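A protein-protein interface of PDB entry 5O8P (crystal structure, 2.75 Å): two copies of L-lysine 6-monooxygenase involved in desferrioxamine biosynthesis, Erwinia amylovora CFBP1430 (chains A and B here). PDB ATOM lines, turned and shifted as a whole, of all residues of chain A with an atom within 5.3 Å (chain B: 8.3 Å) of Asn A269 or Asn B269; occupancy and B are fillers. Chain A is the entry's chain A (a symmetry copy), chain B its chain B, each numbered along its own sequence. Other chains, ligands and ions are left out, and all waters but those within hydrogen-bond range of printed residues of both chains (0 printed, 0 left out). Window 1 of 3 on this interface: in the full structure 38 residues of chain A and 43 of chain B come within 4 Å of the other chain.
The side-chain carboxylate of Glu B235 is in salt-bridge range of the guanidinium group of Arg A230, at 2.8 Å.
The guanidinium group (NH1) of Arg B230 lies within salt-bridge range of the side-chain carboxylate (OE1) of Glu A235 (2.8 Å).
The backbone NH of Glu A235 sits at hydrogen-bond distance from the backbone carbonyl oxygen of Asn A269, at 2.8 Å.
The backbone carbonyl oxygen (O) of Asn B269 is in hydrogen-bond range of the backbone NH (N) of Glu B235.
OE2 of Glu B235 sits at hydrogen-bond distance from OG1 of Thr B240 (2.7 Å).
Thr B240 touches Arg A230.
Arg A230 touches Met B243 (CD to SD, 3.6 Å).
Arg A230 touches Asn B269 (NH2 to ND2, 3.5 Å).
Arg A230 touches Leu B270 (CD to CD2, 3.9 Å).
Tyr A232 touches Glu B235.
CD of Pro A233 touches OE2 of Glu B235, at 3.6 Å.
OE2 of Glu A235 touches CD of Pro B233, at 3.2 Å.
ND2 of Asn A269 touches ND2 of Asn B269, at 3.996 Å.
Of the printed residues of chain B, Asn A269 touches Asn B269 (3.996 Å).
Printed residues of chain A within 4 Å of Asn B269: Arg A230 and Asn A269.
Of the printed residues of chain B, Tyr A232 touches Glu B235.
Of the printed residues of chain B, Glu A235 touches Arg B230 (2.8 Å) and Pro B233 (3.2 Å).
The nearest printed residue of chain A that does not touch Asn B269 is Glu A235 (5.8 Å).
Hydrophobic or aromatic side chains of chain A within 4 Å of the printed part of chain B: Pro A233.
Among the printed residues, Asp or Glu carboxylates within 4 Å of a Lys or Arg side-chain nitrogen of the other chain: Arg A230 with Glu B235 (2.8 Å) and Glu A235 with Arg B230 (2.8 Å).
Arg A230 touches Leu B270, but with the chains exchanged Leu A270 does not touch Arg B230 (4.4 Å).
Tyr A232 touches Glu B235, but with the chains exchanged Glu A235 does not touch Tyr B232 (4.1 Å).
Pro A233 touches Glu B235, and with the chains exchanged Glu A235 touches Pro B233.
Asn A269 touches its own counterpart, Asn B269.
Positions printed for both chains: 230, 232, 233, 234, 235, 267, 268, 269, 270, 271, 272 and 273.
Of the 10 pairs that touch across the chains among the printed residues, 5 have their exchanged pair printed and touching as well.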
ATOM      1  N   ARG A 230     -12.975  -1.517  11.403  1.00  0.00           N
ATOM      2  CA  ARG A 230     -13.913  -2.624  11.488  1.00  0.00           C
ATOM      3  C   ARG A 230     -13.689  -3.324  12.806  1.00  0.00           C
ATOM      4  O   ARG A 230     -12.762  -2.977  13.535  1.00  0.00           O
ATOM      5  CB  ARG A 230     -13.655  -3.610  10.350  1.00  0.00           C
ATOM      6  CG  ARG A 230     -13.854  -3.061   8.947  1.00  0.00           C
ATOM      7  CD  ARG A 230     -13.626  -4.171   7.937  1.00  0.00           C
ATOM      8  NE  ARG A 230     -12.245  -4.648   8.018  1.00  0.00           N
ATOM      9  CZ  ARG A 230     -11.191  -4.027   7.494  1.00  0.00           C
ATOM     10  NH1 ARG A 230     -11.323  -2.895   6.787  1.00  0.00           N
ATOM     11  NH2 ARG A 230      -9.985  -4.562   7.659  1.00  0.00           N
ATOM     12  N   TYR A 232     -12.103  -6.022  13.181  1.00  0.00           N
ATOM     13  CA  TYR A 232     -11.266  -6.878  12.338  1.00  0.00           C
ATOM     14  C   TYR A 232     -10.827  -8.091  13.141  1.00  0.00           C
ATOM     15  O   TYR A 232     -10.553  -7.984  14.339  1.00  0.00           O
ATOM     16  CB  TYR A 232     -10.066  -6.155  11.668  1.00  0.00           C
ATOM     17  CG  TYR A 232      -9.233  -5.229  12.527  1.00  0.00           C
ATOM     18  CD1 TYR A 232      -8.507  -5.707  13.631  1.00  0.00           C
ATOM     19  CD2 TYR A 232      -9.132  -3.866  12.215  1.00  0.00           C
ATOM     20  CE1 TYR A 232      -7.755  -4.852  14.429  1.00  0.00           C
ATOM     21  CE2 TYR A 232      -8.373  -3.000  13.006  1.00  0.00           C
ATOM     22  CZ  TYR A 232      -7.681  -3.496  14.115  1.00  0.00           C
ATOM     23  OH  TYR A 232      -6.914  -2.659  14.918  1.00  0.00           O
ATOM     24  N   PRO A 233     -10.805  -9.267  12.495  1.00  0.00           N
ATOM     25  CA  PRO A 233     -10.258 -10.429  13.167  1.00  0.00           C
ATOM     26  C   PRO A 233      -8.732 -10.417  13.177  1.00  0.00           C
ATOM     27  O   PRO A 233      -8.090  -9.741  12.352  1.00  0.00           O
ATOM     28  CB  PRO A 233     -10.766 -11.592  12.320  1.00  0.00           C
ATOM     29  CG  PRO A 233     -10.860 -11.023  10.944  1.00  0.00           C
ATOM     30  CD  PRO A 233     -11.258  -9.589  11.126  1.00  0.00           C
ATOM     31  N   LEU A 234      -8.175 -11.168  14.117  1.00  0.00           N
ATOM     32  CA  LEU A 234      -6.756 -11.423  14.174  1.00  0.00           C
ATOM     33  C   LEU A 234      -6.445 -12.331  12.990  1.00  0.00           C
ATOM     34  O   LEU A 234      -7.102 -13.358  12.839  1.00  0.00           O
ATOM     35  CB  LEU A 234      -6.429 -12.120  15.489  1.00  0.00           C
ATOM     36  CG  LEU A 234      -4.949 -12.422  15.721  1.00  0.00           C
ATOM     37  CD1 LEU A 234      -4.218 -11.140  16.148  1.00  0.00           C
ATOM     38  CD2 LEU A 234      -4.771 -13.560  16.722  1.00  0.00           C
ATOM     39  N   GLU A 235      -5.478 -11.944  12.154  1.00  0.00           N
ATOM     40  CA  GLU A 235      -5.151 -12.684  10.919  1.00  0.00           C
ATOM     41  C   GLU A 235      -4.362 -13.953  11.269  1.00  0.00           C
ATOM     42  O   GLU A 235      -3.243 -13.883  11.768  1.00  0.00           O
ATOM     43  CB  GLU A 235      -4.376 -11.819   9.905  1.00  0.00           C
ATOM     44  CG  GLU A 235      -4.418 -12.362   8.481  1.00  0.00           C
ATOM     45  CD  GLU A 235      -3.982 -11.368   7.415  1.00  0.00           C
ATOM     46  OE1 GLU A 235      -4.385 -10.178   7.476  1.00  0.00           O
ATOM     47  OE2 GLU A 235      -3.264 -11.769   6.483  1.00  0.00           O
ATOM     48  N   GLN A 267      -0.496  -2.736  10.558  1.00  0.00           N
ATOM     49  CA  GLN A 267      -0.327  -4.179  10.786  1.00  0.00           C
ATOM     50  C   GLN A 267      -1.130  -4.646  12.019  1.00  0.00           C
ATOM     51  O   GLN A 267      -0.752  -5.614  12.676  1.00  0.00           O
ATOM     52  CB  GLN A 267       1.160  -4.539  10.936  1.00  0.00           C
ATOM     53  CG  GLN A 267       1.936  -4.661   9.624  1.00  0.00           C
ATOM     54  CD  GLN A 267       3.360  -5.186   9.839  1.00  0.00           C
ATOM     55  OE1 GLN A 267       3.947  -5.000  10.912  1.00  0.00           O
ATOM     56  NE2 GLN A 267       3.908  -5.867   8.831  1.00  0.00           N
ATOM     57  N   LYS A 268      -2.218  -3.943  12.335  1.00  0.00           N
ATOM     58  CA  LYS A 268      -2.976  -4.214  13.555  1.00  0.00           C
ATOM     59  C   LYS A 268      -3.819  -5.493  13.488  1.00  0.00           C
ATOM     60  O   LYS A 268      -4.095  -6.092  14.532  1.00  0.00           O
ATOM     61  CB  LYS A 268      -3.803  -2.994  13.969  1.00  0.00           C
ATOM     62  CG  LYS A 268      -2.941  -1.779  14.286  1.00  0.00           C
ATOM     63  CD  LYS A 268      -3.654  -0.733  15.114  1.00  0.00           C
ATOM     64  CE  LYS A 268      -2.685   0.398  15.419  1.00  0.00           C
ATOM     65  NZ  LYS A 268      -3.361   1.570  16.026  1.00  0.00           N
ATOM     66  N   ASN A 269      -4.210  -5.921  12.274  1.00  0.00           N
ATOM     67  CA  ASN A 269      -4.772  -7.281  12.025  1.00  0.00           C
ATOM     68  C   ASN A 269      -3.884  -8.418  12.574  1.00  0.00           C
ATOM     69  O   ASN A 269      -4.390  -9.470  12.987  1.00  0.00           O
ATOM     70  CB  ASN A 269      -4.897  -7.617  10.514  1.00  0.00           C
ATOM     71  CG  ASN A 269      -5.611  -6.562   9.693  1.00  0.00           C
ATOM     72  OD1 ASN A 269      -6.114  -5.567  10.210  1.00  0.00           O
ATOM     73  ND2 ASN A 269      -5.643  -6.783   8.383  1.00  0.00           N
ATOM     74  N   LEU A 270      -2.567  -8.218  12.533  1.00  0.00           N
ATOM     75  CA  LEU A 270      -1.600  -9.264  12.878  1.00  0.00           C
ATOM     76  C   LEU A 270      -1.375  -9.450  14.393  1.00  0.00           C
ATOM     77  O   LEU A 270      -0.909 -10.510  14.809  1.00  0.00           O
ATOM     78  CB  LEU A 270      -0.265  -8.992  12.171  1.00  0.00           C
ATOM     79  CG  LEU A 270      -0.163  -8.998  10.630  1.00  0.00           C
ATOM     80  CD1 LEU A 270      -1.434  -8.696   9.838  1.00  0.00           C
ATOM     81  CD2 LEU A 270       0.962  -8.091  10.140  1.00  0.00           C
ATOM     82  N   TYR A 271      -1.696  -8.437  15.205  1.00  0.00           N
ATOM     83  CA  TYR A 271      -1.545  -8.535  16.677  1.00  0.00           C
ATOM     84  C   TYR A 271      -2.692  -7.968  17.545  1.00  0.00           C
ATOM     85  O   TYR A 271      -2.957  -8.525  18.607  1.00  0.00           O
ATOM     86  CB  TYR A 271      -0.172  -7.984  17.134  1.00  0.00           C
ATOM     87  CG  TYR A 271       0.074  -6.477  17.007  1.00  0.00           C
ATOM     88  CD1 TYR A 271       0.076  -5.848  15.761  1.00  0.00           C
ATOM     89  CD2 TYR A 271       0.345  -5.684  18.136  1.00  0.00           C
ATOM     90  CE1 TYR A 271       0.334  -4.478  15.630  1.00  0.00           C
ATOM     91  CE2 TYR A 271       0.583  -4.315  18.016  1.00  0.00           C
ATOM     92  CZ  TYR A 271       0.580  -3.720  16.757  1.00  0.00           C
ATOM     93  OH  TYR A 271       0.823  -2.378  16.613  1.00  0.00           O
ATOM     94  N   LYS A 272      -3.371  -6.906  17.100  1.00  0.00           N
ATOM     95  CA  LYS A 272      -4.445  -6.243  17.877  1.00  0.00           C
ATOM     96  C   LYS A 272      -5.883  -6.703  17.490  1.00  0.00           C
ATOM     97  O   LYS A 272      -6.866  -6.047  17.858  1.00  0.00           O
ATOM     98  CB  LYS A 272      -4.246  -4.702  17.784  1.00  0.00           C
ATOM     99  CG  LYS A 272      -5.420  -3.729  17.993  1.00  0.00           C
ATOM    100  CD  LYS A 272      -6.003  -3.756  19.406  1.00  0.00           C
ATOM    101  CE  LYS A 272      -5.408  -2.680  20.300  1.00  0.00           C
ATOM    102  NZ  LYS A 272      -6.052  -2.688  21.640  1.00  0.00           N
ATOM    103  N   GLY A 273      -6.018  -7.833  16.797  1.00  0.00           N
ATOM    104  CA  GLY A 273      -7.330  -8.298  16.361  1.00  0.00           C
ATOM    105  C   GLY A 273      -8.128  -9.116  17.374  1.00  0.00           C
ATOM    106  O   GLY A 273      -7.634  -9.513  18.428  1.00  0.00           O
ATOM    107  N   ARG B 230       0.924  -8.918   1.643  1.00  0.00           N
ATOM    108  CA  ARG B 230       0.827 -10.286   2.120  1.00  0.00           C
ATOM    109  C   ARG B 230      -0.089 -11.032   1.170  1.00  0.00           C
ATOM    110  O   ARG B 230      -0.658 -10.432   0.251  1.00  0.00           O
ATOM    111  CB  ARG B 230       0.185 -10.308   3.506  1.00  0.00           C
ATOM    112  CG  ARG B 230       0.975  -9.591   4.600  1.00  0.00           C
ATOM    113  CD  ARG B 230       0.114  -9.121   5.766  1.00  0.00           C
ATOM    114  NE  ARG B 230      -0.644  -7.943   5.370  1.00  0.00           N
ATOM    115  CZ  ARG B 230      -1.974  -7.842   5.326  1.00  0.00           C
ATOM    116  NH1 ARG B 230      -2.761  -8.857   5.687  1.00  0.00           N
ATOM    117  NH2 ARG B 230      -2.524  -6.705   4.902  1.00  0.00           N
ATOM    118  N   TYR B 232      -3.150 -11.855   1.550  1.00  0.00           N
ATOM    119  CA  TYR B 232      -4.207 -11.549   2.514  1.00  0.00           C
ATOM    120  C   TYR B 232      -5.458 -12.366   2.234  1.00  0.00           C
ATOM    121  O   TYR B 232      -5.810 -12.589   1.079  1.00  0.00           O
ATOM    122  CB  TYR B 232      -4.529 -10.035   2.634  1.00  0.00           C
ATOM    123  CG  TYR B 232      -4.713  -9.241   1.350  1.00  0.00           C
ATOM    124  CD1 TYR B 232      -5.771  -9.517   0.482  1.00  0.00           C
ATOM    125  CD2 TYR B 232      -3.850  -8.184   1.023  1.00  0.00           C
ATOM    126  CE1 TYR B 232      -5.963  -8.788  -0.693  1.00  0.00           C
ATOM    127  CE2 TYR B 232      -4.030  -7.449  -0.150  1.00  0.00           C
ATOM    128  CZ  TYR B 232      -5.088  -7.755  -1.012  1.00  0.00           C
ATOM    129  OH  TYR B 232      -5.279  -7.045  -2.183  1.00  0.00           O
ATOM    130  N   PRO B 233      -6.110 -12.855   3.295  1.00  0.00           N
ATOM    131  CA  PRO B 233      -7.392 -13.514   3.098  1.00  0.00           C
ATOM    132  C   PRO B 233      -8.529 -12.518   2.879  1.00  0.00           C
ATOM    133  O   PRO B 233      -8.436 -11.355   3.270  1.00  0.00           O
ATOM    134  CB  PRO B 233      -7.600 -14.272   4.410  1.00  0.00           C
ATOM    135  CG  PRO B 233      -6.914 -13.435   5.416  1.00  0.00           C
ATOM    136  CD  PRO B 233      -5.734 -12.821   4.719  1.00  0.00           C
ATOM    137  N   LEU B 234      -9.589 -13.009   2.257  1.00  0.00           N
ATOM    138  CA  LEU B 234     -10.836 -12.296   2.118  1.00  0.00           C
ATOM    139  C   LEU B 234     -11.443 -12.261   3.507  1.00  0.00           C
ATOM    140  O   LEU B 234     -11.566 -13.320   4.131  1.00  0.00           O
ATOM    141  CB  LEU B 234     -11.764 -13.059   1.175  1.00  0.00           C
ATOM    142  CG  LEU B 234     -13.106 -12.416   0.875  1.00  0.00           C
ATOM    143  CD1 LEU B 234     -12.904 -11.306  -0.130  1.00  0.00           C
ATOM    144  CD2 LEU B 234     -14.101 -13.452   0.354  1.00  0.00           C
ATOM    145  N   GLU B 235     -11.806 -11.070   4.001  1.00  0.00           N
ATOM    146  CA  GLU B 235     -12.392 -10.945   5.343  1.00  0.00           C
ATOM    147  C   GLU B 235     -13.854 -11.431   5.385  1.00  0.00           C
ATOM    148  O   GLU B 235     -14.737 -10.833   4.775  1.00  0.00           O
ATOM    149  CB  GLU B 235     -12.268  -9.517   5.859  1.00  0.00           C
ATOM    150  CG  GLU B 235     -12.397  -9.401   7.397  1.00  0.00           C
ATOM    151  CD  GLU B 235     -11.821  -8.077   7.927  1.00  0.00           C
ATOM    152  OE1 GLU B 235     -10.675  -7.739   7.580  1.00  0.00           O
ATOM    153  OE2 GLU B 235     -12.531  -7.352   8.672  1.00  0.00           O
ATOM    154  N   TYR B 236     -14.084 -12.520   6.103  1.00  0.00           N
ATOM    155  CA  TYR B 236     -15.365 -13.247   6.082  1.00  0.00           C
ATOM    156  C   TYR B 236     -16.025 -13.393   7.470  1.00  0.00           C
ATOM    157  O   TYR B 236     -17.030 -14.119   7.657  1.00  0.00           O
ATOM    158  CB  TYR B 236     -15.191 -14.625   5.430  1.00  0.00           C
ATOM    159  CG  TYR B 236     -16.419 -15.129   4.690  1.00  0.00           C
ATOM    160  CD1 TYR B 236     -16.838 -14.514   3.501  1.00  0.00           C
ATOM    161  CD2 TYR B 236     -17.149 -16.242   5.154  1.00  0.00           C
ATOM    162  CE1 TYR B 236     -17.962 -14.971   2.815  1.00  0.00           C
ATOM    163  CE2 TYR B 236     -18.268 -16.716   4.465  1.00  0.00           C
ATOM    164  CZ  TYR B 236     -18.677 -16.081   3.291  1.00  0.00           C
ATOM    165  OH  TYR B 236     -19.794 -16.528   2.596  1.00  0.00           O
ATOM    166  N   THR B 240     -17.971  -8.025   9.800  1.00  0.00           N
ATOM    167  CA  THR B 240     -17.526  -7.376   8.542  1.00  0.00           C
ATOM    168  C   THR B 240     -18.480  -7.673   7.377  1.00  0.00           C
ATOM    169  O   THR B 240     -18.693  -6.802   6.538  1.00  0.00           O
ATOM    170  CB  THR B 240     -16.077  -7.769   8.162  1.00  0.00           C
ATOM    171  OG1 THR B 240     -15.196  -7.335   9.197  1.00  0.00           O
ATOM    172  CG2 THR B 240     -15.643  -7.148   6.851  1.00  0.00           C
ATOM    173  N   MET B 243     -21.077  -5.157   6.344  1.00  0.00           N
ATOM    174  CA  MET B 243     -20.748  -4.051   5.445  1.00  0.00           C
ATOM    175  C   MET B 243     -21.274  -4.285   4.033  1.00  0.00           C
ATOM    176  O   MET B 243     -21.331  -3.333   3.271  1.00  0.00           O
ATOM    177  CB  MET B 243     -19.238  -3.799   5.398  1.00  0.00           C
ATOM    178  CG  MET B 243     -18.628  -3.358   6.713  1.00  0.00           C
ATOM    179  SD  MET B 243     -16.825  -3.256   6.675  1.00  0.00           S
ATOM    180  CE  MET B 243     -16.585  -1.683   5.866  1.00  0.00           C
ATOM    181  N   LEU B 263     -10.788   4.692  -0.168  1.00  0.00           N
ATOM    182  CA  LEU B 263     -11.403   3.517   0.468  1.00  0.00           C
ATOM    183  C   LEU B 263     -11.310   2.249  -0.392  1.00  0.00           C
ATOM    184  O   LEU B 263     -11.085   1.183   0.121  1.00  0.00           O
ATOM    185  CB  LEU B 263     -12.877   3.763   0.846  1.00  0.00           C
ATOM    186  CG  LEU B 263     -13.127   4.191   2.296  1.00  0.00           C
ATOM    187  CD1 LEU B 263     -12.780   3.050   3.247  1.00  0.00           C
ATOM    188  CD2 LEU B 263     -12.372   5.451   2.685  1.00  0.00           C
ATOM    189  N   ASN B 264     -11.510   2.371  -1.695  1.00  0.00           N
ATOM    190  CA  ASN B 264     -11.512   1.191  -2.581  1.00  0.00           C
ATOM    191  C   ASN B 264     -10.126   0.543  -2.748  1.00  0.00           C
ATOM    192  O   ASN B 264     -10.041  -0.659  -2.947  1.00  0.00           O
ATOM    193  CB  ASN B 264     -12.176   1.514  -3.929  1.00  0.00           C
ATOM    194  CG  ASN B 264     -13.706   1.602  -3.821  1.00  0.00           C
ATOM    195  OD1 ASN B 264     -14.349   0.899  -3.012  1.00  0.00           O
ATOM    196  ND2 ASN B 264     -14.298   2.484  -4.624  1.00  0.00           N
ATOM    197  N   ALA B 265      -9.060   1.337  -2.657  1.00  0.00           N
ATOM    198  CA  ALA B 265      -7.690   0.830  -2.612  1.00  0.00           C
ATOM    199  C   ALA B 265      -7.246   0.252  -1.251  1.00  0.00           C
ATOM    200  O   ALA B 265      -6.396  -0.641  -1.229  1.00  0.00           O
ATOM    201  CB  ALA B 265      -6.692   1.876  -3.109  1.00  0.00           C
ATOM    202  N   SER B 266      -7.799   0.741  -0.139  1.00  0.00           N
ATOM    203  CA  SER B 266      -7.478   0.210   1.199  1.00  0.00           C
ATOM    204  C   SER B 266      -8.397  -0.926   1.696  1.00  0.00           C
ATOM    205  O   SER B 266      -8.193  -1.447   2.792  1.00  0.00           O
ATOM    206  CB  SER B 266      -7.436   1.360   2.227  1.00  0.00           C
ATOM    207  OG  SER B 266      -8.725   1.712   2.712  1.00  0.00           O
ATOM    208  N   GLN B 267      -9.434  -1.257   0.926  1.00  0.00           N
ATOM    209  CA  GLN B 267     -10.450  -2.249   1.339  1.00  0.00           C
ATOM    210  C   GLN B 267     -10.395  -3.449   0.393  1.00  0.00           C
ATOM    211  O   GLN B 267     -11.413  -4.094   0.133  1.00  0.00           O
ATOM    212  CB  GLN B 267     -11.881  -1.654   1.351  1.00  0.00           C
ATOM    213  CG  GLN B 267     -12.206  -0.713   2.500  1.00  0.00           C
ATOM    214  CD  GLN B 267     -13.641  -0.220   2.489  1.00  0.00           C
ATOM    215  OE1 GLN B 267     -14.298  -0.152   1.442  1.00  0.00           O
ATOM    216  NE2 GLN B 267     -14.121   0.174   3.656  1.00  0.00           N
ATOM    217  N   LYS B 268      -9.196  -3.807  -0.057  1.00  0.00           N
ATOM    218  CA  LYS B 268      -9.029  -4.966  -0.938  1.00  0.00           C
ATOM    219  C   LYS B 268      -9.185  -6.316  -0.200  1.00  0.00           C
ATOM    220  O   LYS B 268      -9.553  -7.297  -0.838  1.00  0.00           O
ATOM    221  CB  LYS B 268      -7.690  -4.882  -1.679  1.00  0.00           C
ATOM    222  CG  LYS B 268      -7.625  -3.680  -2.608  1.00  0.00           C
ATOM    223  CD  LYS B 268      -6.271  -3.563  -3.279  1.00  0.00           C
ATOM    224  CE  LYS B 268      -6.271  -2.534  -4.395  1.00  0.00           C
ATOM    225  NZ  LYS B 268      -5.178  -2.805  -5.366  1.00  0.00           N
ATOM    226  N   ASN B 269      -8.930  -6.366   1.115  1.00  0.00           N
ATOM    227  CA  ASN B 269      -9.293  -7.575   1.903  1.00  0.00           C
ATOM    228  C   ASN B 269     -10.805  -7.890   1.907  1.00  0.00           C
ATOM    229  O   ASN B 269     -11.186  -9.042   2.108  1.00  0.00           O
ATOM    230  CB  ASN B 269      -8.665  -7.651   3.326  1.00  0.00           C
ATOM    231  CG  ASN B 269      -8.764  -6.363   4.117  1.00  0.00           C
ATOM    232  OD1 ASN B 269      -9.400  -5.394   3.711  1.00  0.00           O
ATOM    233  ND2 ASN B 269      -8.106  -6.349   5.266  1.00  0.00           N
ATOM    234  N   LEU B 270     -11.651  -6.885   1.661  1.00  0.00           N
ATOM    235  CA  LEU B 270     -13.102  -7.074   1.656  1.00  0.00           C
ATOM    236  C   LEU B 270     -13.668  -7.684   0.359  1.00  0.00           C
ATOM    237  O   LEU B 270     -14.766  -8.248   0.379  1.00  0.00           O
ATOM    238  CB  LEU B 270     -13.823  -5.749   1.977  1.00  0.00           C
ATOM    239  CG  LEU B 270     -13.551  -5.008   3.306  1.00  0.00           C
ATOM    240  CD1 LEU B 270     -14.653  -3.994   3.584  1.00  0.00           C
ATOM    241  CD2 LEU B 270     -13.357  -5.958   4.483  1.00  0.00           C
ATOM    242  N   TYR B 271     -12.944  -7.566  -0.756  1.00  0.00           N
ATOM    243  CA  TYR B 271     -13.406  -8.128  -2.053  1.00  0.00           C
ATOM    244  C   TYR B 271     -12.350  -8.840  -2.930  1.00  0.00           C
ATOM    245  O   TYR B 271     -12.691  -9.811  -3.606  1.00  0.00           O
ATOM    246  CB  TYR B 271     -14.201  -7.089  -2.877  1.00  0.00           C
ATOM    247  CG  TYR B 271     -13.427  -5.897  -3.445  1.00  0.00           C
ATOM    248  CD1 TYR B 271     -12.811  -4.966  -2.599  1.00  0.00           C
ATOM    249  CD2 TYR B 271     -13.377  -5.659  -4.830  1.00  0.00           C
ATOM    250  CE1 TYR B 271     -12.131  -3.874  -3.103  1.00  0.00           C
ATOM    251  CE2 TYR B 271     -12.700  -4.554  -5.348  1.00  0.00           C
ATOM    252  CZ  TYR B 271     -12.083  -3.664  -4.478  1.00  0.00           C
ATOM    253  OH  TYR B 271     -11.405  -2.565  -4.954  1.00  0.00           O
ATOM    254  N   LYS B 272     -11.092  -8.386  -2.901  1.00  0.00           N
ATOM    255  CA  LYS B 272     -10.009  -8.957  -3.730  1.00  0.00           C
ATOM    256  C   LYS B 272      -9.113  -9.981  -2.978  1.00  0.00           C
ATOM    257  O   LYS B 272      -8.018 -10.291  -3.408  1.00  0.00           O
ATOM    258  CB  LYS B 272      -9.189  -7.796  -4.341  1.00  0.00           C
ATOM    259  CG  LYS B 272      -9.852  -7.133  -5.549  1.00  0.00           C
ATOM    260  CD  LYS B 272      -9.411  -5.678  -5.768  1.00  0.00           C
ATOM    261  CE  LYS B 272      -7.891  -5.446  -5.802  1.00  0.00           C
ATOM    262  NZ  LYS B 272      -7.139  -6.166  -6.874  1.00  0.00           N
ATOM    263  N   GLY B 273      -9.595 -10.536  -1.867  1.00  0.00           N
ATOM    264  CA  GLY B 273      -8.810 -11.487  -1.064  1.00  0.00           C
ATOM    265  C   GLY B 273      -8.904 -12.929  -1.519  1.00  0.00           C
ATOM    266  O   GLY B 273      -9.742 -13.272  -2.347  1.00  0.00           O
ATOM    267  N   ILE B 274      -8.053 -13.770  -0.940  1.00  0.00           N
ATOM    268  CA  ILE B 274      -8.104 -15.214  -1.140  1.00  0.00           C
ATOM    269  C   ILE B 274      -8.946 -15.857  -0.034  1.00  0.00           C
ATOM    270  O   ILE B 274      -8.915 -15.420   1.108  1.00  0.00           O
ATOM    271  CB  ILE B 274      -6.699 -15.836  -1.093  1.00  0.00           C
ATOM    272  CG1 ILE B 274      -5.750 -15.140  -2.067  1.00  0.00           C
ATOM    273  CG2 ILE B 274      -6.763 -17.315  -1.428  1.00  0.00           C
ATOM    274  CD1 ILE B 274      -4.288 -15.401  -1.784  1.00  0.00           C
ATOM    275  N   PHE B 391     -16.880  -1.585  -2.388  1.00  0.00           N
ATOM    276  CA  PHE B 391     -16.423  -2.981  -2.556  1.00  0.00           C
ATOM    277  C   PHE B 391     -17.520  -4.047  -2.804  1.00  0.00           C
ATOM    278  O   PHE B 391     -17.185  -5.201  -3.113  1.00  0.00           O
ATOM    279  CB  PHE B 391     -15.611  -3.380  -1.318  1.00  0.00           C
ATOM    280  CG  PHE B 391     -16.459  -3.866  -0.172  1.00  0.00           C
ATOM    281  CD1 PHE B 391     -17.040  -2.980   0.734  1.00  0.00           C
ATOM    282  CD2 PHE B 391     -16.737  -5.224  -0.055  1.00  0.00           C
ATOM    283  CE1 PHE B 391     -17.834  -3.451   1.761  1.00  0.00           C
ATOM    284  CE2 PHE B 391     -17.541  -5.701   0.961  1.00  0.00           C
ATOM    285  CZ  PHE B 391     -18.077  -4.816   1.875  1.00  0.00           C
